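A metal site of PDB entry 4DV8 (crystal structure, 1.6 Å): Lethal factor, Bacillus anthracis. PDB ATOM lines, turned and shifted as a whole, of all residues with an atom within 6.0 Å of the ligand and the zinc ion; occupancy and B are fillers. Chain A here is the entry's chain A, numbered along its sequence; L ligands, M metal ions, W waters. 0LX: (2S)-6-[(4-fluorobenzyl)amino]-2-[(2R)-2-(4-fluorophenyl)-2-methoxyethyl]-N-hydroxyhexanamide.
The zinc ion is bound by the side-chain carboxylate (OE1) of Glu 485 (2.1 Å). A ring nitrogen (NE2) of His 440 is bound to the zinc ion, 2.1 Å away. The zinc ion is bound by O04 of the ligand. NE2 of His 436 is bound to the zinc ion (2.2 Å). O01 of the ligand binds the zinc ion (2.2 Å). The zinc ion has five donor atoms within binding distance.
Water W2 lies within hydrogen-bond range of the backbone NH of Tyr 409 (2.9 Å) and a nitrogen (N03) of the ligand (3.3 Å). Water W1 bridges OE2 of Glu 412 and OE1 of Gln 396.
A fluorine (F29) of the ligand lies close to the backbone NH (N) of Glu 426 (3.3 Å). Asp 78 touches the ligand (O to C06, 3.7 Å). Gln 392 touches the ligand (CG to F18, 3.7 Å). Gln 396 touches the ligand. Val 403 touches the ligand. Ser 405 touches the ligand. Lys 406 touches the ligand (CB to C22, 3.7 Å). Leu 408 touches the ligand (CD2 to F18, 3.5 Å). O of Tyr 409 touches C14 of the ligand (3.4 Å). Val 410 touches the ligand (CG2 to F18, 3.4 Å). Gly 424 touches the ligand (CA to C27, 3.8 Å). N of Val 425 touches C27 of the ligand, 3.9 Å away. Leu 427 touches the ligand (CG to C26, 3.4 Å). Glu 489 touches the ligand (OE2 to C25, 3.4 Å). Hydrophobic or aromatic side chains within 4 Å of the ligand: Val 403, Leu 408, Val 410, Leu 427, His 436, His 440 and Tyr 478. 20 residues have an atom within 4 Å of the ligand: Asp 78, Gln 392, Gln 396, Val 403, Ser 405, Lys 406, Gly 407, Leu 408, Tyr 409, Val 410, Gly 424, Val 425, Glu 426, Leu 427, His 436, Glu 437, His 440, Tyr 478, Glu 485 and Glu 489.
The nearest printed residue that does not touch the zinc ion is Tyr 478 (4.05 Å).
The side-chain carboxylate of Glu 489 is in salt-bridge range of the guanidinium group of Arg 492 (2.7 Å). The backbone NH (N) of Leu 408 lies close to the side-chain carboxylate (OE1) of Glu 437 (3.3 Å). OE1 of Glu 426 sits at hydrogen-bond distance from N of Tyr 478 (3.0 Å). The backbone carbonyl oxygen (O) of Gln 396 sits at hydrogen-bond distance from the side-chain amide nitrogen (NE2) of Gln 402 (3.0 Å). OE2 of Glu 489 is in hydrogen-bond range of ND1 of His 436 (2.8 Å). OH of Tyr 478 sits close to OE2 of Glu 485, 3.4 Å away. The backbone carbonyl oxygen of Gly 407 is in hydrogen-bond range of the side-chain hydroxyl of Ser 405 (2.8 Å). The backbone NH (N) of Val 403 lies within hydrogen-bond range of the side-chain amide oxygen (OE1) of Gln 392, 2.8 Å away.
O21 of the ligand is in hydrogen-bond range of N of Gly 407 (3.4 Å). N03 of the ligand sits at hydrogen-bond distance from O of Gly 407 (2.9 Å). The side-chain hydroxyl of Tyr 478 sits close to an oxygen (O01) of the ligand. The side-chain carboxylate (OE1) of Glu 437 sits at hydrogen-bond distance from a nitrogen (N03) of the ligand.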
ATOM      1  N   ASP A  78      15.027 -12.879  -8.446  1.00  0.00           N
ATOM      2  CA  ASP A  78      15.660 -13.862  -7.561  1.00  0.00           C
ATOM      3  C   ASP A  78      14.829 -15.135  -7.369  1.00  0.00           C
ATOM      4  O   ASP A  78      15.195 -15.994  -6.584  1.00  0.00           O
ATOM      5  CB  ASP A  78      16.016 -13.230  -6.205  1.00  0.00           C
ATOM      6  CG  ASP A  78      14.830 -12.598  -5.511  1.00  0.00           C
ATOM      7  OD1 ASP A  78      13.691 -13.044  -5.751  1.00  0.00           O
ATOM      8  OD2 ASP A  78      15.029 -11.654  -4.710  1.00  0.00           O
ATOM      9  N   PHE A  79      13.738 -15.271  -8.130  1.00  0.00           N
ATOM     10  CA  PHE A  79      12.762 -16.337  -7.870  1.00  0.00           C
ATOM     11  C   PHE A  79      12.407 -17.220  -9.053  1.00  0.00           C
ATOM     12  O   PHE A  79      11.623 -18.168  -8.910  1.00  0.00           O
ATOM     13  CB  PHE A  79      11.480 -15.724  -7.310  1.00  0.00           C
ATOM     14  CG  PHE A  79      10.907 -14.638  -8.172  1.00  0.00           C
ATOM     15  CD1 PHE A  79       9.945 -14.942  -9.131  1.00  0.00           C
ATOM     16  CD2 PHE A  79      11.320 -13.331  -8.041  1.00  0.00           C
ATOM     17  CE1 PHE A  79       9.414 -13.932  -9.936  1.00  0.00           C
ATOM     18  CE2 PHE A  79      10.799 -12.323  -8.835  1.00  0.00           C
ATOM     19  CZ  PHE A  79       9.842 -12.622  -9.788  1.00  0.00           C
ATOM     20  N   GLU A 391       8.218 -28.599   2.521  1.00  0.00           N
ATOM     21  CA  GLU A 391       8.553 -27.570   3.508  1.00  0.00           C
ATOM     22  C   GLU A 391       8.383 -26.150   2.950  1.00  0.00           C
ATOM     23  O   GLU A 391       8.226 -25.203   3.730  1.00  0.00           O
ATOM     24  CB  GLU A 391       9.971 -27.797   4.083  1.00  0.00           C
ATOM     25  CG  GLU A 391      10.081 -28.973   5.036  1.00  0.00           C
ATOM     26  CD  GLU A 391      10.183 -30.331   4.346  1.00  0.00           C
ATOM     27  OE1 GLU A 391      10.214 -30.380   3.102  1.00  0.00           O
ATOM     28  OE2 GLU A 391      10.228 -31.364   5.065  1.00  0.00           O
ATOM     29  N   GLN A 392       8.421 -25.983   1.624  1.00  0.00           N
ATOM     30  CA  GLN A 392       7.968 -24.735   1.014  1.00  0.00           C
ATOM     31  C   GLN A 392       6.485 -24.733   0.623  1.00  0.00           C
ATOM     32  O   GLN A 392       5.739 -23.861   1.071  1.00  0.00           O
ATOM     33  CB  GLN A 392       8.809 -24.319  -0.210  1.00  0.00           C
ATOM     34  CG  GLN A 392       8.294 -22.986  -0.757  1.00  0.00           C
ATOM     35  CD  GLN A 392       8.970 -22.432  -2.005  1.00  0.00           C
ATOM     36  OE1 GLN A 392       8.709 -21.290  -2.379  1.00  0.00           O
ATOM     37  NE2 GLN A 392       9.826 -23.232  -2.664  1.00  0.00           N
ATOM     38  N   GLN A 396       3.412 -21.937   1.041  1.00  0.00           N
ATOM     39  CA  GLN A 396       3.177 -21.007  -0.054  1.00  0.00           C
ATOM     40  C   GLN A 396       2.166 -21.629  -1.012  1.00  0.00           C
ATOM     41  O   GLN A 396       2.563 -22.269  -1.997  1.00  0.00           O
ATOM     42  CB  GLN A 396       4.487 -20.701  -0.800  1.00  0.00           C
ATOM     43  CG  GLN A 396       5.691 -20.367   0.090  1.00  0.00           C
ATOM     44  CD  GLN A 396       5.673 -18.942   0.631  1.00  0.00           C
ATOM     45  OE1 GLN A 396       5.463 -18.714   1.817  1.00  0.00           O
ATOM     46  NE2 GLN A 396       5.925 -17.977  -0.247  1.00  0.00           N
ATOM     47  N   GLU A 401       3.834 -17.080  -5.411  1.00  0.00           N
ATOM     48  CA  GLU A 401       4.729 -16.845  -4.269  1.00  0.00           C
ATOM     49  C   GLU A 401       5.769 -17.961  -4.063  1.00  0.00           C
ATOM     50  O   GLU A 401       6.653 -17.835  -3.201  1.00  0.00           O
ATOM     51  CB  GLU A 401       3.940 -16.638  -2.981  1.00  0.00           C
ATOM     52  CG  GLU A 401       3.027 -15.420  -2.979  1.00  0.00           C
ATOM     53  CD  GLU A 401       3.779 -14.079  -2.929  1.00  0.00           C
ATOM     54  OE1 GLU A 401       3.098 -13.056  -2.764  1.00  0.00           O
ATOM     55  OE2 GLU A 401       5.022 -14.032  -3.081  1.00  0.00           O
ATOM     56  N   GLN A 402       5.649 -19.040  -4.830  1.00  0.00           N
ATOM     57  CA  GLN A 402       6.630 -20.117  -4.756  1.00  0.00           C
ATOM     58  C   GLN A 402       7.909 -19.717  -5.494  1.00  0.00           C
ATOM     59  O   GLN A 402       7.876 -18.993  -6.512  1.00  0.00           O
ATOM     60  CB  GLN A 402       6.043 -21.410  -5.335  1.00  0.00           C
ATOM     61  CG  GLN A 402       4.882 -21.943  -4.518  1.00  0.00           C
ATOM     62  CD  GLN A 402       4.217 -23.111  -5.195  1.00  0.00           C
ATOM     63  OE1 GLN A 402       4.573 -23.451  -6.323  1.00  0.00           O
ATOM     64  NE2 GLN A 402       3.227 -23.709  -4.528  1.00  0.00           N
ATOM     65  N   VAL A 403       9.035 -20.168  -4.967  1.00  0.00           N
ATOM     66  CA  VAL A 403      10.319 -19.693  -5.440  1.00  0.00           C
ATOM     67  C   VAL A 403      11.258 -20.821  -5.838  1.00  0.00           C
ATOM     68  O   VAL A 403      11.325 -21.849  -5.139  1.00  0.00           O
ATOM     69  CB  VAL A 403      10.976 -18.869  -4.301  1.00  0.00           C
ATOM     70  CG1 VAL A 403      12.424 -18.585  -4.596  1.00  0.00           C
ATOM     71  CG2 VAL A 403      10.197 -17.562  -4.100  1.00  0.00           C
ATOM     72  N   HIS A 404      11.963 -20.712  -6.955  1.00  0.00           N
ATOM     73  CA  HIS A 404      13.126 -21.578  -7.090  1.00  0.00           C
ATOM     74  C   HIS A 404      14.351 -20.712  -6.966  1.00  0.00           C
ATOM     75  O   HIS A 404      14.403 -19.584  -7.481  1.00  0.00           O
ATOM     76  CB  HIS A 404      13.142 -22.437  -8.366  1.00  0.00           C
ATOM     77  CG  HIS A 404      14.260 -23.441  -8.409  1.00  0.00           C
ATOM     78  ND1 HIS A 404      14.566 -24.280  -7.344  1.00  0.00           N
ATOM     79  CD2 HIS A 404      15.146 -23.742  -9.379  1.00  0.00           C
ATOM     80  CE1 HIS A 404      15.588 -25.045  -7.674  1.00  0.00           C
ATOM     81  NE2 HIS A 404      15.968 -24.741  -8.905  1.00  0.00           N
ATOM     82  N   SER A 405      15.319 -21.248  -6.257  1.00  0.00           N
ATOM     83  CA  SER A 405      16.552 -20.559  -5.866  1.00  0.00           C
ATOM     84  C   SER A 405      17.569 -21.571  -5.341  1.00  0.00           C
ATOM     85  O   SER A 405      17.232 -22.736  -5.105  1.00  0.00           O
ATOM     86  CB  SER A 405      16.257 -19.520  -4.780  1.00  0.00           C
ATOM     87  OG  SER A 405      15.656 -20.120  -3.647  1.00  0.00           O
ATOM     88  N   LYS A 406      18.809 -21.124  -5.125  1.00  0.00           N
ATOM     89  CA  LYS A 406      19.840 -22.009  -4.607  1.00  0.00           C
ATOM     90  C   LYS A 406      19.491 -22.515  -3.215  1.00  0.00           C
ATOM     91  O   LYS A 406      19.746 -23.685  -2.873  1.00  0.00           O
ATOM     92  CB  LYS A 406      21.191 -21.275  -4.581  1.00  0.00           C
ATOM     93  CG  LYS A 406      22.326 -22.070  -3.915  1.00  0.00           C
ATOM     94  CD  LYS A 406      22.612 -23.340  -4.722  1.00  0.00           C
ATOM     95  CE  LYS A 406      23.568 -24.230  -3.965  1.00  0.00           C
ATOM     96  NZ  LYS A 406      23.891 -25.465  -4.767  1.00  0.00           N
ATOM     97  N   GLY A 407      18.909 -21.646  -2.406  1.00  0.00           N
ATOM     98  CA  GLY A 407      18.478 -22.026  -1.070  1.00  0.00           C
ATOM     99  C   GLY A 407      17.323 -21.180  -0.572  1.00  0.00           C
ATOM    100  O   GLY A 407      17.006 -20.146  -1.153  1.00  0.00           O
ATOM    101  N   LEU A 408      16.701 -21.618   0.510  1.00  0.00           N
ATOM    102  CA  LEU A 408      15.563 -20.913   1.061  1.00  0.00           C
ATOM    103  C   LEU A 408      15.506 -21.147   2.563  1.00  0.00           C
ATOM    104  O   LEU A 408      15.966 -22.178   3.061  1.00  0.00           O
ATOM    105  CB  LEU A 408      14.277 -21.465   0.432  1.00  0.00           C
ATOM    106  CG  LEU A 408      13.053 -20.594   0.248  1.00  0.00           C
ATOM    107  CD1 LEU A 408      13.361 -19.292  -0.495  1.00  0.00           C
ATOM    108  CD2 LEU A 408      12.012 -21.414  -0.540  1.00  0.00           C
ATOM    109  N   TYR A 409      14.919 -20.207   3.280  1.00  0.00           N
ATOM    110  CA  TYR A 409      14.528 -20.437   4.661  1.00  0.00           C
ATOM    111  C   TYR A 409      13.043 -20.162   4.788  1.00  0.00           C
ATOM    112  O   TYR A 409      12.588 -19.061   4.474  1.00  0.00           O
ATOM    113  CB  TYR A 409      15.332 -19.569   5.656  1.00  0.00           C
ATOM    114  CG  TYR A 409      14.816 -19.761   7.077  1.00  0.00           C
ATOM    115  CD1 TYR A 409      15.056 -20.936   7.759  1.00  0.00           C
ATOM    116  CD2 TYR A 409      14.027 -18.792   7.693  1.00  0.00           C
ATOM    117  CE1 TYR A 409      14.549 -21.155   9.024  1.00  0.00           C
ATOM    118  CE2 TYR A 409      13.517 -18.994   8.976  1.00  0.00           C
ATOM    119  CZ  TYR A 409      13.780 -20.178   9.635  1.00  0.00           C
ATOM    120  OH  TYR A 409      13.285 -20.430  10.889  1.00  0.00           O
ATOM    121  N   VAL A 410      12.295 -21.172   5.236  1.00  0.00           N
ATOM    122  CA  VAL A 410      10.858 -21.033   5.377  1.00  0.00           C
ATOM    123  C   VAL A 410      10.489 -20.937   6.852  1.00  0.00           C
ATOM    124  O   VAL A 410      10.508 -21.926   7.569  1.00  0.00           O
ATOM    125  CB  VAL A 410      10.119 -22.234   4.759  1.00  0.00           C
ATOM    126  CG1 VAL A 410       8.624 -22.002   4.784  1.00  0.00           C
ATOM    127  CG2 VAL A 410      10.601 -22.467   3.326  1.00  0.00           C
ATOM    128  N   PRO A 411      10.155 -19.722   7.322  1.00  0.00           N
ATOM    129  CA  PRO A 411       9.903 -19.584   8.759  1.00  0.00           C
ATOM    130  C   PRO A 411       8.746 -20.449   9.228  1.00  0.00           C
ATOM    131  O   PRO A 411       8.781 -20.966  10.344  1.00  0.00           O
ATOM    132  CB  PRO A 411       9.556 -18.101   8.921  1.00  0.00           C
ATOM    133  CG  PRO A 411      10.087 -17.427   7.667  1.00  0.00           C
ATOM    134  CD  PRO A 411       9.943 -18.464   6.588  1.00  0.00           C
ATOM    135  N   GLU A 412       7.729 -20.633   8.384  1.00  0.00           N
ATOM    136  CA  GLU A 412       6.551 -21.388   8.784  1.00  0.00           C
ATOM    137  C   GLU A 412       6.832 -22.871   9.061  1.00  0.00           C
ATOM    138  O   GLU A 412       6.102 -23.511   9.829  1.00  0.00           O
ATOM    139  CB  GLU A 412       5.435 -21.251   7.751  1.00  0.00           C
ATOM    140  CG  GLU A 412       4.855 -19.846   7.604  1.00  0.00           C
ATOM    141  CD  GLU A 412       5.603 -18.966   6.602  1.00  0.00           C
ATOM    142  OE1 GLU A 412       5.106 -17.867   6.317  1.00  0.00           O
ATOM    143  OE2 GLU A 412       6.691 -19.360   6.119  1.00  0.00           O
ATOM    144  N   LEU A 418      18.151 -26.504   0.502  1.00  0.00           N
ATOM    145  CA  LEU A 418      19.329 -26.248  -0.302  1.00  0.00           C
ATOM    146  C   LEU A 418      19.303 -27.108  -1.549  1.00  0.00           C
ATOM    147  O   LEU A 418      19.329 -28.340  -1.476  1.00  0.00           O
ATOM    148  CB  LEU A 418      20.604 -26.519   0.515  1.00  0.00           C
ATOM    149  CG  LEU A 418      21.939 -25.962   0.017  1.00  0.00           C
ATOM    150  CD1 LEU A 418      21.951 -24.448   0.089  1.00  0.00           C
ATOM    151  CD2 LEU A 418      23.112 -26.529   0.813  1.00  0.00           C
ATOM    152  N   GLY A 424      24.415 -20.323  -6.827  1.00  0.00           N
ATOM    153  CA  GLY A 424      24.084 -18.949  -6.493  1.00  0.00           C
ATOM    154  C   GLY A 424      25.095 -18.031  -7.146  1.00  0.00           C
ATOM    155  O   GLY A 424      26.298 -18.304  -7.116  1.00  0.00           O
ATOM    156  N   VAL A 425      24.610 -16.937  -7.732  1.00  0.00           N
ATOM    157  CA  VAL A 425      25.477 -16.041  -8.513  1.00  0.00           C
ATOM    158  C   VAL A 425      26.688 -15.489  -7.735  1.00  0.00           C
ATOM    159  O   VAL A 425      27.821 -15.556  -8.224  1.00  0.00           O
ATOM    160  CB  VAL A 425      24.676 -14.883  -9.149  1.00  0.00           C
ATOM    161  CG1 VAL A 425      25.559 -14.108 -10.120  1.00  0.00           C
ATOM    162  CG2 VAL A 425      23.453 -15.422  -9.873  1.00  0.00           C
ATOM    163  N   GLU A 426      26.459 -14.954  -6.541  1.00  0.00           N
ATOM    164  CA  GLU A 426      27.559 -14.381  -5.761  1.00  0.00           C
ATOM    165  C   GLU A 426      28.103 -15.354  -4.711  1.00  0.00           C
ATOM    166  O   GLU A 426      28.753 -14.928  -3.749  1.00  0.00           O
ATOM    167  CB  GLU A 426      27.133 -13.072  -5.089  1.00  0.00           C
ATOM    168  CG  GLU A 426      26.834 -11.911  -6.047  1.00  0.00           C
ATOM    169  CD  GLU A 426      26.423 -10.633  -5.319  1.00  0.00           C
ATOM    170  OE1 GLU A 426      25.230 -10.510  -4.946  1.00  0.00           O
ATOM    171  OE2 GLU A 426      27.284  -9.761  -5.130  1.00  0.00           O
ATOM    172  N   LEU A 427      27.856 -16.645  -4.894  1.00  0.00           N
ATOM    173  CA  LEU A 427      28.308 -17.661  -3.948  1.00  0.00           C
ATOM    174  C   LEU A 427      29.333 -18.580  -4.603  1.00  0.00           C
ATOM    175  O   LEU A 427      29.146 -19.018  -5.736  1.00  0.00           O
ATOM    176  CB  LEU A 427      27.133 -18.513  -3.449  1.00  0.00           C
ATOM    177  CG  LEU A 427      25.943 -17.843  -2.780  1.00  0.00           C
ATOM    178  CD1 LEU A 427      24.827 -18.853  -2.541  1.00  0.00           C
ATOM    179  CD2 LEU A 427      26.346 -17.190  -1.471  1.00  0.00           C
ATOM    180  N   GLY A 433      25.854 -20.862   0.610  1.00  0.00           N
ATOM    181  CA  GLY A 433      24.413 -20.818   0.499  1.00  0.00           C
ATOM    182  C   GLY A 433      23.737 -21.277   1.775  1.00  0.00           C
ATOM    183  O   GLY A 433      22.770 -20.657   2.219  1.00  0.00           O
ATOM    184  N   PHE A 434      24.226 -22.365   2.367  1.00  0.00           N
ATOM    185  CA  PHE A 434      23.611 -22.881   3.588  1.00  0.00           C
ATOM    186  C   PHE A 434      23.752 -21.856   4.706  1.00  0.00           C
ATOM    187  O   PHE A 434      22.824 -21.647   5.490  1.00  0.00           O
ATOM    188  CB  PHE A 434      24.245 -24.208   3.994  1.00  0.00           C
ATOM    189  CG  PHE A 434      23.552 -24.863   5.160  1.00  0.00           C
ATOM    190  CD1 PHE A 434      22.448 -25.675   4.958  1.00  0.00           C
ATOM    191  CD2 PHE A 434      23.990 -24.652   6.466  1.00  0.00           C
ATOM    192  CE1 PHE A 434      21.796 -26.280   6.030  1.00  0.00           C
ATOM    193  CE2 PHE A 434      23.344 -25.241   7.536  1.00  0.00           C
ATOM    194  CZ  PHE A 434      22.248 -26.065   7.324  1.00  0.00           C
ATOM    195  N   HIS A 436      24.083 -18.602   4.419  1.00  0.00           N
ATOM    196  CA  HIS A 436      23.102 -17.576   4.143  1.00  0.00           C
ATOM    197  C   HIS A 436      21.725 -17.948   4.713  1.00  0.00           C
ATOM    198  O   HIS A 436      21.100 -17.148   5.404  1.00  0.00           O
ATOM    199  CB  HIS A 436      23.025 -17.338   2.628  1.00  0.00           C
ATOM    200  CG  HIS A 436      21.966 -16.364   2.230  1.00  0.00           C
ATOM    201  ND1 HIS A 436      22.233 -15.027   1.982  1.00  0.00           N
ATOM    202  CD2 HIS A 436      20.644 -16.522   2.008  1.00  0.00           C
ATOM    203  CE1 HIS A 436      21.122 -14.411   1.648  1.00  0.00           C
ATOM    204  NE2 HIS A 436      20.135 -15.298   1.652  1.00  0.00           N
ATOM    205  N   GLU A 437      21.245 -19.172   4.451  1.00  0.00           N
ATOM    206  CA  GLU A 437      19.942 -19.554   4.979  1.00  0.00           C
ATOM    207  C   GLU A 437      19.941 -19.593   6.496  1.00  0.00           C
ATOM    208  O   GLU A 437      18.930 -19.229   7.106  1.00  0.00           O
ATOM    209  CB  GLU A 437      19.459 -20.898   4.427  1.00  0.00           C
ATOM    210  CG  GLU A 437      19.537 -21.043   2.912  1.00  0.00           C
ATOM    211  CD  GLU A 437      18.906 -19.911   2.168  1.00  0.00           C
ATOM    212  OE1 GLU A 437      19.301 -19.695   1.007  1.00  0.00           O
ATOM    213  OE2 GLU A 437      18.022 -19.204   2.719  1.00  0.00           O
ATOM    214  N   HIS A 440      19.077 -16.364   7.969  1.00  0.00           N
ATOM    215  CA  HIS A 440      17.652 -16.122   8.109  1.00  0.00           C
ATOM    216  C   HIS A 440      17.076 -16.773   9.364  1.00  0.00           C
ATOM    217  O   HIS A 440      16.192 -16.213  10.011  1.00  0.00           O
ATOM    218  CB  HIS A 440      16.897 -16.694   6.917  1.00  0.00           C
ATOM    219  CG  HIS A 440      17.034 -15.888   5.653  1.00  0.00           C
ATOM    220  ND1 HIS A 440      16.831 -14.542   5.612  1.00  0.00           N
ATOM    221  CD2 HIS A 440      17.321 -16.292   4.393  1.00  0.00           C
ATOM    222  CE1 HIS A 440      16.998 -14.115   4.359  1.00  0.00           C
ATOM    223  NE2 HIS A 440      17.282 -15.155   3.620  1.00  0.00           N
ATOM    224  N   TYR A 478      23.177  -8.545  -3.943  1.00  0.00           N
ATOM    225  CA  TYR A 478      21.960  -9.223  -3.532  1.00  0.00           C
ATOM    226  C   TYR A 478      21.499  -8.730  -2.151  1.00  0.00           C
ATOM    227  O   TYR A 478      20.298  -8.669  -1.869  1.00  0.00           O
ATOM    228  CB  TYR A 478      22.096 -10.750  -3.578  1.00  0.00           C
ATOM    229  CG  TYR A 478      20.829 -11.431  -3.132  1.00  0.00           C
ATOM    230  CD1 TYR A 478      19.650 -11.246  -3.834  1.00  0.00           C
ATOM    231  CD2 TYR A 478      20.804 -12.220  -1.998  1.00  0.00           C
ATOM    232  CE1 TYR A 478      18.474 -11.841  -3.428  1.00  0.00           C
ATOM    233  CE2 TYR A 478      19.625 -12.838  -1.587  1.00  0.00           C
ATOM    234  CZ  TYR A 478      18.463 -12.625  -2.307  1.00  0.00           C
ATOM    235  OH  TYR A 478      17.290 -13.183  -1.903  1.00  0.00           O
ATOM    236  N   ALA A 484      15.912  -8.364   5.288  1.00  0.00           N
ATOM    237  CA  ALA A 484      16.187  -9.759   5.615  1.00  0.00           C
ATOM    238  C   ALA A 484      17.365 -10.288   4.820  1.00  0.00           C
ATOM    239  O   ALA A 484      18.207 -10.996   5.361  1.00  0.00           O
ATOM    240  CB  ALA A 484      14.941 -10.619   5.375  1.00  0.00           C
ATOM    241  N   GLU A 485      17.409  -9.969   3.533  1.00  0.00           N
ATOM    242  CA  GLU A 485      18.501 -10.461   2.711  1.00  0.00           C
ATOM    243  C   GLU A 485      19.826  -9.814   3.072  1.00  0.00           C
ATOM    244  O   GLU A 485      20.858 -10.471   3.052  1.00  0.00           O
ATOM    245  CB  GLU A 485      18.215 -10.263   1.222  1.00  0.00           C
ATOM    246  CG  GLU A 485      16.933 -10.974   0.752  1.00  0.00           C
ATOM    247  CD  GLU A 485      16.902 -12.438   1.109  1.00  0.00           C
ATOM    248  OE1 GLU A 485      17.986 -13.026   1.327  1.00  0.00           O
ATOM    249  OE2 GLU A 485      15.792 -13.015   1.160  1.00  0.00           O
ATOM    250  N   ALA A 488      21.100 -11.541   6.174  1.00  0.00           N
ATOM    251  CA  ALA A 488      21.581 -12.877   5.868  1.00  0.00           C
ATOM    252  C   ALA A 488      22.908 -12.834   5.140  1.00  0.00           C
ATOM    253  O   ALA A 488      23.800 -13.655   5.391  1.00  0.00           O
ATOM    254  CB  ALA A 488      20.533 -13.656   5.039  1.00  0.00           C
ATOM    255  N   GLU A 489      23.051 -11.852   4.249  1.00  0.00           N
ATOM    256  CA  GLU A 489      24.289 -11.673   3.506  1.00  0.00           C
ATOM    257  C   GLU A 489      25.417 -11.201   4.428  1.00  0.00           C
ATOM    258  O   GLU A 489      26.530 -11.729   4.369  1.00  0.00           O
ATOM    259  CB  GLU A 489      24.082 -10.688   2.350  1.00  0.00           C
ATOM    260  CG  GLU A 489      23.414 -11.321   1.117  1.00  0.00           C
ATOM    261  CD  GLU A 489      24.304 -12.357   0.456  1.00  0.00           C
ATOM    262  OE1 GLU A 489      25.048 -11.986  -0.473  1.00  0.00           O
ATOM    263  OE2 GLU A 489      24.285 -13.519   0.889  1.00  0.00           O
ATOM    264  N   ARG A 492      26.422 -14.159   6.481  1.00  0.00           N
ATOM    265  CA  ARG A 492      27.224 -15.123   5.724  1.00  0.00           C
ATOM    266  C   ARG A 492      28.663 -14.660   5.568  1.00  0.00           C
ATOM    267  O   ARG A 492      29.615 -15.424   5.781  1.00  0.00           O
ATOM    268  CB  ARG A 492      26.589 -15.399   4.357  1.00  0.00           C
ATOM    269  CG  ARG A 492      27.595 -15.882   3.330  1.00  0.00           C
ATOM    270  CD  ARG A 492      26.986 -16.065   1.974  1.00  0.00           C
ATOM    271  NE  ARG A 492      26.814 -14.828   1.186  1.00  0.00           N
ATOM    272  CZ  ARG A 492      27.719 -14.347   0.337  1.00  0.00           C
ATOM    273  NH1 ARG A 492      28.899 -14.951   0.193  1.00  0.00           N
ATOM    274  NH2 ARG A 492      27.465 -13.256  -0.356  1.00  0.00           N
HETATM  275  O01 0LX L   1      17.749 -15.385  -0.594  1.00  0.00           O
HETATM  276  C02 0LX L   1      17.546 -16.530  -0.916  1.00  0.00           C
HETATM  277  N03 0LX L   1      17.417 -17.545   0.060  1.00  0.00           N
HETATM  278  O04 0LX L   1      17.351 -17.208   1.352  1.00  0.00           O
HETATM  279  C05 0LX L   1      17.553 -16.878  -2.373  1.00  0.00           C
HETATM  280  C06 0LX L   1      16.485 -16.175  -3.098  1.00  0.00           C
HETATM  281  C07 0LX L   1      15.094 -16.665  -2.629  1.00  0.00           C
HETATM  282  C08 0LX L   1      14.113 -15.523  -2.525  1.00  0.00           C
HETATM  283  C09 0LX L   1      12.829 -15.902  -1.756  1.00  0.00           C
HETATM  284  N10 0LX L   1      12.605 -14.988  -0.595  1.00  0.00           N
HETATM  285  C11 0LX L   1      11.218 -14.983  -0.203  1.00  0.00           C
HETATM  286  C12 0LX L   1      10.727 -16.319   0.207  1.00  0.00           C
HETATM  287  C13 0LX L   1      11.165 -16.924   1.404  1.00  0.00           C
HETATM  288  C14 0LX L   1      10.692 -18.204   1.774  1.00  0.00           C
HETATM  289  C15 0LX L   1       9.763 -18.851   0.951  1.00  0.00           C
HETATM  290  C16 0LX L   1       9.317 -18.248  -0.240  1.00  0.00           C
HETATM  291  C17 0LX L   1       9.795 -16.976  -0.607  1.00  0.00           C
HETATM  292  F18 0LX L   1       9.296 -20.053   1.258  1.00  0.00           F
HETATM  293  C19 0LX L   1      18.968 -16.529  -2.936  1.00  0.00           C
HETATM  294  C20 0LX L   1      20.080 -17.135  -2.114  1.00  0.00           C
HETATM  295  O21 0LX L   1      20.191 -18.503  -2.249  1.00  0.00           O
HETATM  296  C22 0LX L   1      21.137 -19.184  -1.502  1.00  0.00           C
HETATM  297  C23 0LX L   1      21.397 -16.526  -2.539  1.00  0.00           C
HETATM  298  C24 0LX L   1      22.120 -15.778  -1.612  1.00  0.00           C
HETATM  299  C25 0LX L   1      23.304 -15.174  -1.974  1.00  0.00           C
HETATM  300  C26 0LX L   1      23.779 -15.295  -3.288  1.00  0.00           C
HETATM  301  C27 0LX L   1      23.076 -16.047  -4.225  1.00  0.00           C
HETATM  302  C28 0LX L   1      21.871 -16.660  -3.857  1.00  0.00           C
HETATM  303  F29 0LX L   1      24.921 -14.693  -3.621  1.00  0.00           F
HETATM  304 ZN    ZN M   1      17.945 -15.126   1.587  1.00  0.00          ZN
HETATM  305  O   HOH W   1       7.552 -18.417   3.720  1.00  0.00           O
HETATM  306  O   HOH W   2      14.829 -17.508   2.146  1.00  0.00           O
HETATM  307  O   HOH W   3      23.905 -12.795  -6.200  1.00  0.00           O
